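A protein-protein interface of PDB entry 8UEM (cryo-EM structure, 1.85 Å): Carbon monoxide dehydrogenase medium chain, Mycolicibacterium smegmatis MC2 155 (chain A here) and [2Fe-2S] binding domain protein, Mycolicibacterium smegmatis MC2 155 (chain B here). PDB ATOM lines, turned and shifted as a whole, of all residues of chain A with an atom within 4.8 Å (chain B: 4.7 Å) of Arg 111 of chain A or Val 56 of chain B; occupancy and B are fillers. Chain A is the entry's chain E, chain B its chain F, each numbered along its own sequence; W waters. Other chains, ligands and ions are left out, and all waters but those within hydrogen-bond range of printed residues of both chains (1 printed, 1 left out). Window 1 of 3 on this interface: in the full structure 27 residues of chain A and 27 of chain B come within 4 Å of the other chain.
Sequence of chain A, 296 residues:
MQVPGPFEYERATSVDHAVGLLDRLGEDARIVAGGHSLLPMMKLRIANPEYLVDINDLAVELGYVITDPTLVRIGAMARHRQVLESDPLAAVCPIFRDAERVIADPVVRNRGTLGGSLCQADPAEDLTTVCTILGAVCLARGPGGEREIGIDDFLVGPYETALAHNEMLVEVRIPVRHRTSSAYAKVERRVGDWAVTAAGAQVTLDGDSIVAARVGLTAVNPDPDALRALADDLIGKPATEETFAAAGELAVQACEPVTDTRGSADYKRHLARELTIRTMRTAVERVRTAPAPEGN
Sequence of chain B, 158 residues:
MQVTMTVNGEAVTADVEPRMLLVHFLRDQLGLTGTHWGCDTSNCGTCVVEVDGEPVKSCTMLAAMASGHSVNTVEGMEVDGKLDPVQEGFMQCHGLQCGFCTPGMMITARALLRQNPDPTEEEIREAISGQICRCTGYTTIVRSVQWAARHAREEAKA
Arg 111 of chain A touches just these residues of chain B: Glu 54, Val 56, Met 61 and Met 65.
Val 56 of chain B touches just these residues of chain A: Val 107 (3.6 Å) and Arg 111 (3.6 Å).
Of the printed residues of chain A, Glu 54 of chain B touches Asn 110 and Arg 111.
Of the printed residues of chain B, Val 107 of chain A touches Val 48 (3.9 Å), Pro 55 (3.4 Å), Val 56 (3.6 Å) and Lys 57 (3.4 Å).
Gly 34 of chain A touches none of the printed residues of chain B.
The nearest printed residue of chain B that does not touch Arg 111 of chain A is Pro 55 of chain B (5.4 Å).
The nearest printed residue of chain A that does not touch Val 56 of chain B is Asn 110 of chain A (4.9 Å).
The nearest printed residue of chain A that does not touch Glu 54 of chain B is Arg 79 of chain A (5.4 Å).
Water W1 lies within hydrogen-bond range of NE2 of His 36 of chain A (2.7 Å), N of Lys 57 of chain B (2.9 Å) and O of Val 107 of chain A (2.9 Å).
Among the printed residues, merely in contact across the chains: Arg 111 of chain A with Met 65 of chain B (3.2 Å), Val 107 of chain A with Lys 57 of chain B (3.4 Å), Val 107 of chain A with Pro 55 of chain B (3.4 Å), Arg 111 of chain A with Glu 54 of chain B (3.5 Å), Arg 111 of chain A with Val 56 of chain B (3.6 Å), Val 107 of chain A with Val 56 of chain B (3.6 Å), Asn 56 of chain A with Met 65 of chain B (3.6 Å), Arg 111 of chain A with Met 61 of chain B (3.8 Å), Ala 33 of chain A with Met 65 of chain B (3.8 Å) and Val 107 of chain A with Val 48 of chain B (3.9 Å).
Of the 12 printed residues of chain A, 5 touch a printed residue of chain B.
Hydrophobic or aromatic side chains of chain A that line the printed part of chain B: Val 107.
Among the printed residues, 12 pairs touch across the chains.
The backbone carbonyl oxygen (O) of Pro 55 of chain B lies within hydrogen-bond range of the side-chain amide nitrogen (ND2) of Asn 110 of chain A (2.9 Å).
OE2 of Glu 54 of chain B lies close to O of Asn 110 of chain A (3.3 Å).
The backbone carbonyl oxygen (O) of Val 49 of chain B is in hydrogen-bond range of the backbone NH (N) of Val 56 of chain B, 2.6 Å away.
The guanidinium group of Arg 79 of chain A sits at hydrogen-bond distance from the side-chain amide oxygen of Asn 56 of chain A (2.8 Å).
The guanidinium group of Arg 79 of chain A lies within hydrogen-bond range of the backbone carbonyl oxygen of Arg 111 of chain A.
The backbone carbonyl oxygen (O) of Ala 33 of chain A sits at hydrogen-bond distance from the side-chain amide nitrogen (ND2) of Asn 56 of chain A (2.6 Å).
The side-chain amide oxygen of Asn 56 of chain A sits at hydrogen-bond distance from the guanidinium group of Arg 111 of chain A, 3.5 Å away.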
ATOM      1  N   ALA A  33       7.815 -15.349   7.350  1.00  0.00           N
ATOM      2  CA  ALA A  33       8.589 -16.456   6.793  1.00  0.00           C
ATOM      3  C   ALA A  33       9.818 -16.568   7.671  1.00  0.00           C
ATOM      4  O   ALA A  33       9.723 -17.057   8.793  1.00  0.00           O
ATOM      5  CB  ALA A  33       8.968 -16.137   5.380  1.00  0.00           C
ATOM      6  N   GLY A  34      10.884 -15.940   7.214  1.00  0.00           N
ATOM      7  CA  GLY A  34      12.105 -16.104   7.964  1.00  0.00           C
ATOM      8  C   GLY A  34      12.072 -15.139   9.120  1.00  0.00           C
ATOM      9  O   GLY A  34      12.777 -15.306  10.112  1.00  0.00           O
ATOM     10  N   HIS A  36      13.240 -12.259   9.248  1.00  0.00           N
ATOM     11  CA  HIS A  36      14.436 -11.441   9.376  1.00  0.00           C
ATOM     12  C   HIS A  36      14.261 -10.039   8.816  1.00  0.00           C
ATOM     13  O   HIS A  36      15.182  -9.225   8.928  1.00  0.00           O
ATOM     14  CB  HIS A  36      15.618 -12.154   8.724  1.00  0.00           C
ATOM     15  CG  HIS A  36      16.225 -13.193   9.610  1.00  0.00           C
ATOM     16  ND1 HIS A  36      15.474 -14.177  10.212  1.00  0.00           N
ATOM     17  CD2 HIS A  36      17.493 -13.366  10.047  1.00  0.00           C
ATOM     18  CE1 HIS A  36      16.257 -14.929  10.962  1.00  0.00           C
ATOM     19  NE2 HIS A  36      17.489 -14.463  10.873  1.00  0.00           N
ATOM     20  N   ASN A  56       6.461 -21.004   7.685  1.00  0.00           N
ATOM     21  CA  ASN A  56       7.690 -21.828   7.757  1.00  0.00           C
ATOM     22  C   ASN A  56       7.378 -23.306   7.520  1.00  0.00           C
ATOM     23  O   ASN A  56       8.282 -24.030   7.131  1.00  0.00           O
ATOM     24  CB  ASN A  56       8.460 -21.606   9.060  1.00  0.00           C
ATOM     25  CG  ASN A  56       9.299 -20.347   9.001  1.00  0.00           C
ATOM     26  OD1 ASN A  56      10.280 -20.278   8.270  1.00  0.00           O
ATOM     27  ND2 ASN A  56       8.919 -19.342   9.765  1.00  0.00           N
ATOM     28  N   ARG A  79      15.095 -20.438   1.320  1.00  0.00           N
ATOM     29  CA  ARG A  79      16.054 -19.714   2.175  1.00  0.00           C
ATOM     30  C   ARG A  79      17.105 -19.070   1.274  1.00  0.00           C
ATOM     31  O   ARG A  79      17.490 -19.666   0.292  1.00  0.00           O
ATOM     32  CB  ARG A  79      16.744 -20.704   3.123  1.00  0.00           C
ATOM     33  CG  ARG A  79      15.766 -21.444   4.021  1.00  0.00           C
ATOM     34  CD  ARG A  79      14.875 -20.532   4.837  1.00  0.00           C
ATOM     35  NE  ARG A  79      13.889 -21.352   5.517  1.00  0.00           N
ATOM     36  CZ  ARG A  79      12.936 -20.917   6.330  1.00  0.00           C
ATOM     37  NH1 ARG A  79      12.819 -19.631   6.614  1.00  0.00           N
ATOM     38  NH2 ARG A  79      12.104 -21.787   6.869  1.00  0.00           N
ATOM     39  N   VAL A 107      24.087 -16.742   8.835  1.00  0.00           N
ATOM     40  CA  VAL A 107      23.009 -17.091   9.754  1.00  0.00           C
ATOM     41  C   VAL A 107      21.687 -16.524   9.253  1.00  0.00           C
ATOM     42  O   VAL A 107      20.669 -17.220   9.222  1.00  0.00           O
ATOM     43  CB  VAL A 107      23.332 -16.614  11.181  1.00  0.00           C
ATOM     44  CG1 VAL A 107      22.242 -17.049  12.134  1.00  0.00           C
ATOM     45  CG2 VAL A 107      24.667 -17.175  11.634  1.00  0.00           C
ATOM     46  N   VAL A 108      21.681 -15.264   8.794  1.00  0.00           N
ATOM     47  CA  VAL A 108      20.434 -14.612   8.268  1.00  0.00           C
ATOM     48  C   VAL A 108      20.013 -15.370   7.017  1.00  0.00           C
ATOM     49  O   VAL A 108      18.835 -15.633   6.851  1.00  0.00           O
ATOM     50  CB  VAL A 108      20.573 -13.108   7.955  1.00  0.00           C
ATOM     51  CG1 VAL A 108      19.333 -12.528   7.293  1.00  0.00           C
ATOM     52  CG2 VAL A 108      20.955 -12.318   9.196  1.00  0.00           C
ATOM     53  N   ARG A 109      20.978 -15.719   6.201  1.00  0.00           N
ATOM     54  CA  ARG A 109      20.670 -16.464   4.963  1.00  0.00           C
ATOM     55  C   ARG A 109      19.996 -17.803   5.274  1.00  0.00           C
ATOM     56  O   ARG A 109      19.287 -18.309   4.409  1.00  0.00           O
ATOM     57  CB  ARG A 109      21.909 -16.586   4.088  1.00  0.00           C
ATOM     58  CG  ARG A 109      22.337 -15.237   3.534  1.00  0.00           C
ATOM     59  CD  ARG A 109      23.259 -15.378   2.350  1.00  0.00           C
ATOM     60  NE  ARG A 109      24.482 -16.067   2.697  1.00  0.00           N
ATOM     61  CZ  ARG A 109      25.598 -15.481   3.101  1.00  0.00           C
ATOM     62  NH1 ARG A 109      25.659 -14.168   3.232  1.00  0.00           N
ATOM     63  NH2 ARG A 109      26.653 -16.219   3.381  1.00  0.00           N
ATOM     64  N   ASN A 110      20.288 -18.361   6.434  1.00  0.00           N
ATOM     65  CA  ASN A 110      19.648 -19.619   6.798  1.00  0.00           C
ATOM     66  C   ASN A 110      18.143 -19.466   6.946  1.00  0.00           C
ATOM     67  O   ASN A 110      17.405 -20.438   6.767  1.00  0.00           O
ATOM     68  CB  ASN A 110      20.249 -20.163   8.091  1.00  0.00           C
ATOM     69  CG  ASN A 110      21.612 -20.744   7.877  1.00  0.00           C
ATOM     70  OD1 ASN A 110      21.983 -21.052   6.753  1.00  0.00           O
ATOM     71  ND2 ASN A 110      22.374 -20.888   8.945  1.00  0.00           N
ATOM     72  N   ARG A 111      17.672 -18.264   7.270  1.00  0.00           N
ATOM     73  CA  ARG A 111      16.265 -18.030   7.558  1.00  0.00           C
ATOM     74  C   ARG A 111      15.577 -17.158   6.521  1.00  0.00           C
ATOM     75  O   ARG A 111      14.521 -17.532   6.008  1.00  0.00           O
ATOM     76  CB  ARG A 111      16.127 -17.399   8.946  1.00  0.00           C
ATOM     77  CG  ARG A 111      16.664 -18.288  10.046  1.00  0.00           C
ATOM     78  CD  ARG A 111      15.795 -19.510  10.204  1.00  0.00           C
ATOM     79  NE  ARG A 111      14.472 -19.132  10.676  1.00  0.00           N
ATOM     80  CZ  ARG A 111      13.377 -19.863  10.533  1.00  0.00           C
ATOM     81  NH1 ARG A 111      13.408 -21.044   9.946  1.00  0.00           N
ATOM     82  NH2 ARG A 111      12.223 -19.392  10.991  1.00  0.00           N
ATOM     83  N   GLY A 112      16.162 -16.011   6.206  1.00  0.00           N
ATOM     84  CA  GLY A 112      15.538 -15.074   5.268  1.00  0.00           C
ATOM     85  C   GLY A 112      15.158 -15.785   4.004  1.00  0.00           C
ATOM     86  O   GLY A 112      15.895 -16.698   3.585  1.00  0.00           O
ATOM     87  N   THR A 113      14.099 -15.324   3.368  1.00  0.00           N
ATOM     88  CA  THR A 113      13.600 -16.045   2.177  1.00  0.00           C
ATOM     89  C   THR A 113      13.470 -15.107   0.991  1.00  0.00           C
ATOM     90  O   THR A 113      13.300 -13.913   1.190  1.00  0.00           O
ATOM     91  CB  THR A 113      12.303 -16.819   2.434  1.00  0.00           C
ATOM     92  OG1 THR A 113      11.261 -15.873   2.664  1.00  0.00           O
ATOM     93  CG2 THR A 113      12.388 -17.797   3.584  1.00  0.00           C
ATOM     94  N   CYS B  47      23.129 -14.481  19.846  1.00  0.00           N
ATOM     95  CA  CYS B  47      21.969 -15.311  20.105  1.00  0.00           C
ATOM     96  C   CYS B  47      21.943 -16.566  19.252  1.00  0.00           C
ATOM     97  O   CYS B  47      20.972 -17.320  19.321  1.00  0.00           O
ATOM     98  CB  CYS B  47      20.710 -14.499  19.832  1.00  0.00           C
ATOM     99  SG  CYS B  47      20.591 -14.099  18.090  1.00  0.00           S
ATOM    100  N   VAL B  48      22.961 -16.791  18.425  1.00  0.00           N
ATOM    101  CA  VAL B  48      22.893 -17.881  17.465  1.00  0.00           C
ATOM    102  C   VAL B  48      22.709 -19.195  18.198  1.00  0.00           C
ATOM    103  O   VAL B  48      23.452 -19.523  19.130  1.00  0.00           O
ATOM    104  CB  VAL B  48      24.140 -17.903  16.576  1.00  0.00           C
ATOM    105  CG1 VAL B  48      24.242 -19.240  15.854  1.00  0.00           C
ATOM    106  CG2 VAL B  48      24.088 -16.757  15.580  1.00  0.00           C
ATOM    107  N   VAL B  49      21.694 -19.943  17.791  1.00  0.00           N
ATOM    108  CA  VAL B  49      21.440 -21.278  18.291  1.00  0.00           C
ATOM    109  C   VAL B  49      21.273 -22.177  17.081  1.00  0.00           C
ATOM    110  O   VAL B  49      21.244 -21.722  15.938  1.00  0.00           O
ATOM    111  CB  VAL B  49      20.198 -21.346  19.207  1.00  0.00           C
ATOM    112  CG1 VAL B  49      20.374 -20.433  20.397  1.00  0.00           C
ATOM    113  CG2 VAL B  49      18.934 -20.991  18.436  1.00  0.00           C
ATOM    114  N   VAL B  51      18.823 -24.383  15.245  1.00  0.00           N
ATOM    115  CA  VAL B  51      17.446 -24.778  14.990  1.00  0.00           C
ATOM    116  C   VAL B  51      17.466 -25.713  13.796  1.00  0.00           C
ATOM    117  O   VAL B  51      17.871 -25.318  12.698  1.00  0.00           O
ATOM    118  CB  VAL B  51      16.538 -23.568  14.726  1.00  0.00           C
ATOM    119  CG1 VAL B  51      15.139 -24.035  14.368  1.00  0.00           C
ATOM    120  CG2 VAL B  51      16.513 -22.651  15.934  1.00  0.00           C
ATOM    121  N   GLU B  54      20.764 -25.843  12.024  1.00  0.00           N
ATOM    122  CA  GLU B  54      21.346 -24.701  11.355  1.00  0.00           C
ATOM    123  C   GLU B  54      21.460 -23.514  12.304  1.00  0.00           C
ATOM    124  O   GLU B  54      20.523 -23.224  13.054  1.00  0.00           O
ATOM    125  CB  GLU B  54      20.513 -24.309  10.127  1.00  0.00           C
ATOM    126  CG  GLU B  54      19.527 -23.182  10.352  1.00  0.00           C
ATOM    127  CD  GLU B  54      18.527 -23.075   9.220  1.00  0.00           C
ATOM    128  OE1 GLU B  54      18.819 -23.610   8.128  1.00  0.00           O
ATOM    129  OE2 GLU B  54      17.458 -22.458   9.412  1.00  0.00           O
ATOM    130  N   PRO B  55      22.595 -22.822  12.305  1.00  0.00           N
ATOM    131  CA  PRO B  55      22.716 -21.623  13.134  1.00  0.00           C
ATOM    132  C   PRO B  55      21.605 -20.645  12.799  1.00  0.00           C
ATOM    133  O   PRO B  55      21.351 -20.340  11.633  1.00  0.00           O
ATOM    134  CB  PRO B  55      24.093 -21.066  12.761  1.00  0.00           C
ATOM    135  CG  PRO B  55      24.819 -22.220  12.184  1.00  0.00           C
ATOM    136  CD  PRO B  55      23.796 -23.051  11.494  1.00  0.00           C
ATOM    137  N   VAL B  56      20.938 -20.168  13.834  1.00  0.00           N
ATOM    138  CA  VAL B  56      19.836 -19.235  13.686  1.00  0.00           C
ATOM    139  C   VAL B  56      19.959 -18.193  14.780  1.00  0.00           C
ATOM    140  O   VAL B  56      20.261 -18.517  15.932  1.00  0.00           O
ATOM    141  CB  VAL B  56      18.468 -19.945  13.756  1.00  0.00           C
ATOM    142  CG1 VAL B  56      17.367 -18.932  13.976  1.00  0.00           C
ATOM    143  CG2 VAL B  56      18.226 -20.762  12.501  1.00  0.00           C
ATOM    144  N   LYS B  57      19.729 -16.944  14.422  1.00  0.00           N
ATOM    145  CA  LYS B  57      19.672 -15.884  15.418  1.00  0.00           C
ATOM    146  C   LYS B  57      18.385 -16.076  16.199  1.00  0.00           C
ATOM    147  O   LYS B  57      17.295 -15.814  15.694  1.00  0.00           O
ATOM    148  CB  LYS B  57      19.755 -14.518  14.749  1.00  0.00           C
ATOM    149  CG  LYS B  57      21.013 -14.387  13.908  1.00  0.00           C
ATOM    150  CD  LYS B  57      21.374 -12.959  13.551  1.00  0.00           C
ATOM    151  CE  LYS B  57      22.846 -12.877  13.183  1.00  0.00           C
ATOM    152  NZ  LYS B  57      23.237 -11.617  12.501  1.00  0.00           N
ATOM    153  N   SER B  58      18.503 -16.593  17.423  1.00  0.00           N
ATOM    154  CA  SER B  58      17.317 -16.851  18.229  1.00  0.00           C
ATOM    155  C   SER B  58      16.578 -15.572  18.578  1.00  0.00           C
ATOM    156  O   SER B  58      15.410 -15.632  18.963  1.00  0.00           O
ATOM    157  CB  SER B  58      17.691 -17.600  19.505  1.00  0.00           C
ATOM    158  OG  SER B  58      18.508 -16.804  20.339  1.00  0.00           O
ATOM    159  N   MET B  61      13.772 -15.161  15.876  1.00  0.00           N
ATOM    160  CA  MET B  61      12.865 -16.287  15.764  1.00  0.00           C
ATOM    161  C   MET B  61      11.950 -16.260  16.972  1.00  0.00           C
ATOM    162  O   MET B  61      12.423 -16.132  18.102  1.00  0.00           O
ATOM    163  CB  MET B  61      13.620 -17.617  15.706  1.00  0.00           C
ATOM    164  CG  MET B  61      12.767 -18.781  15.253  1.00  0.00           C
ATOM    165  SD  MET B  61      13.706 -20.139  14.548  1.00  0.00           S
ATOM    166  CE  MET B  61      12.384 -21.308  14.249  1.00  0.00           C
ATOM    167  N   MET B  65       7.509 -19.994  16.613  1.00  0.00           N
ATOM    168  CA  MET B  65       8.039 -20.466  15.320  1.00  0.00           C
ATOM    169  C   MET B  65       8.941 -21.672  15.545  1.00  0.00           C
ATOM    170  O   MET B  65       8.974 -22.513  14.685  1.00  0.00           O
ATOM    171  CB  MET B  65       8.837 -19.372  14.599  1.00  0.00           C
ATOM    172  CG  MET B  65       7.997 -18.229  14.067  1.00  0.00           C
ATOM    173  SD  MET B  65       8.992 -16.758  13.674  1.00  0.00           S
ATOM    174  CE  MET B  65      10.208 -17.479  12.578  1.00  0.00           C
HETATM  175  O   HOH W   1      19.296 -16.309  11.636  1.00  0.00           O
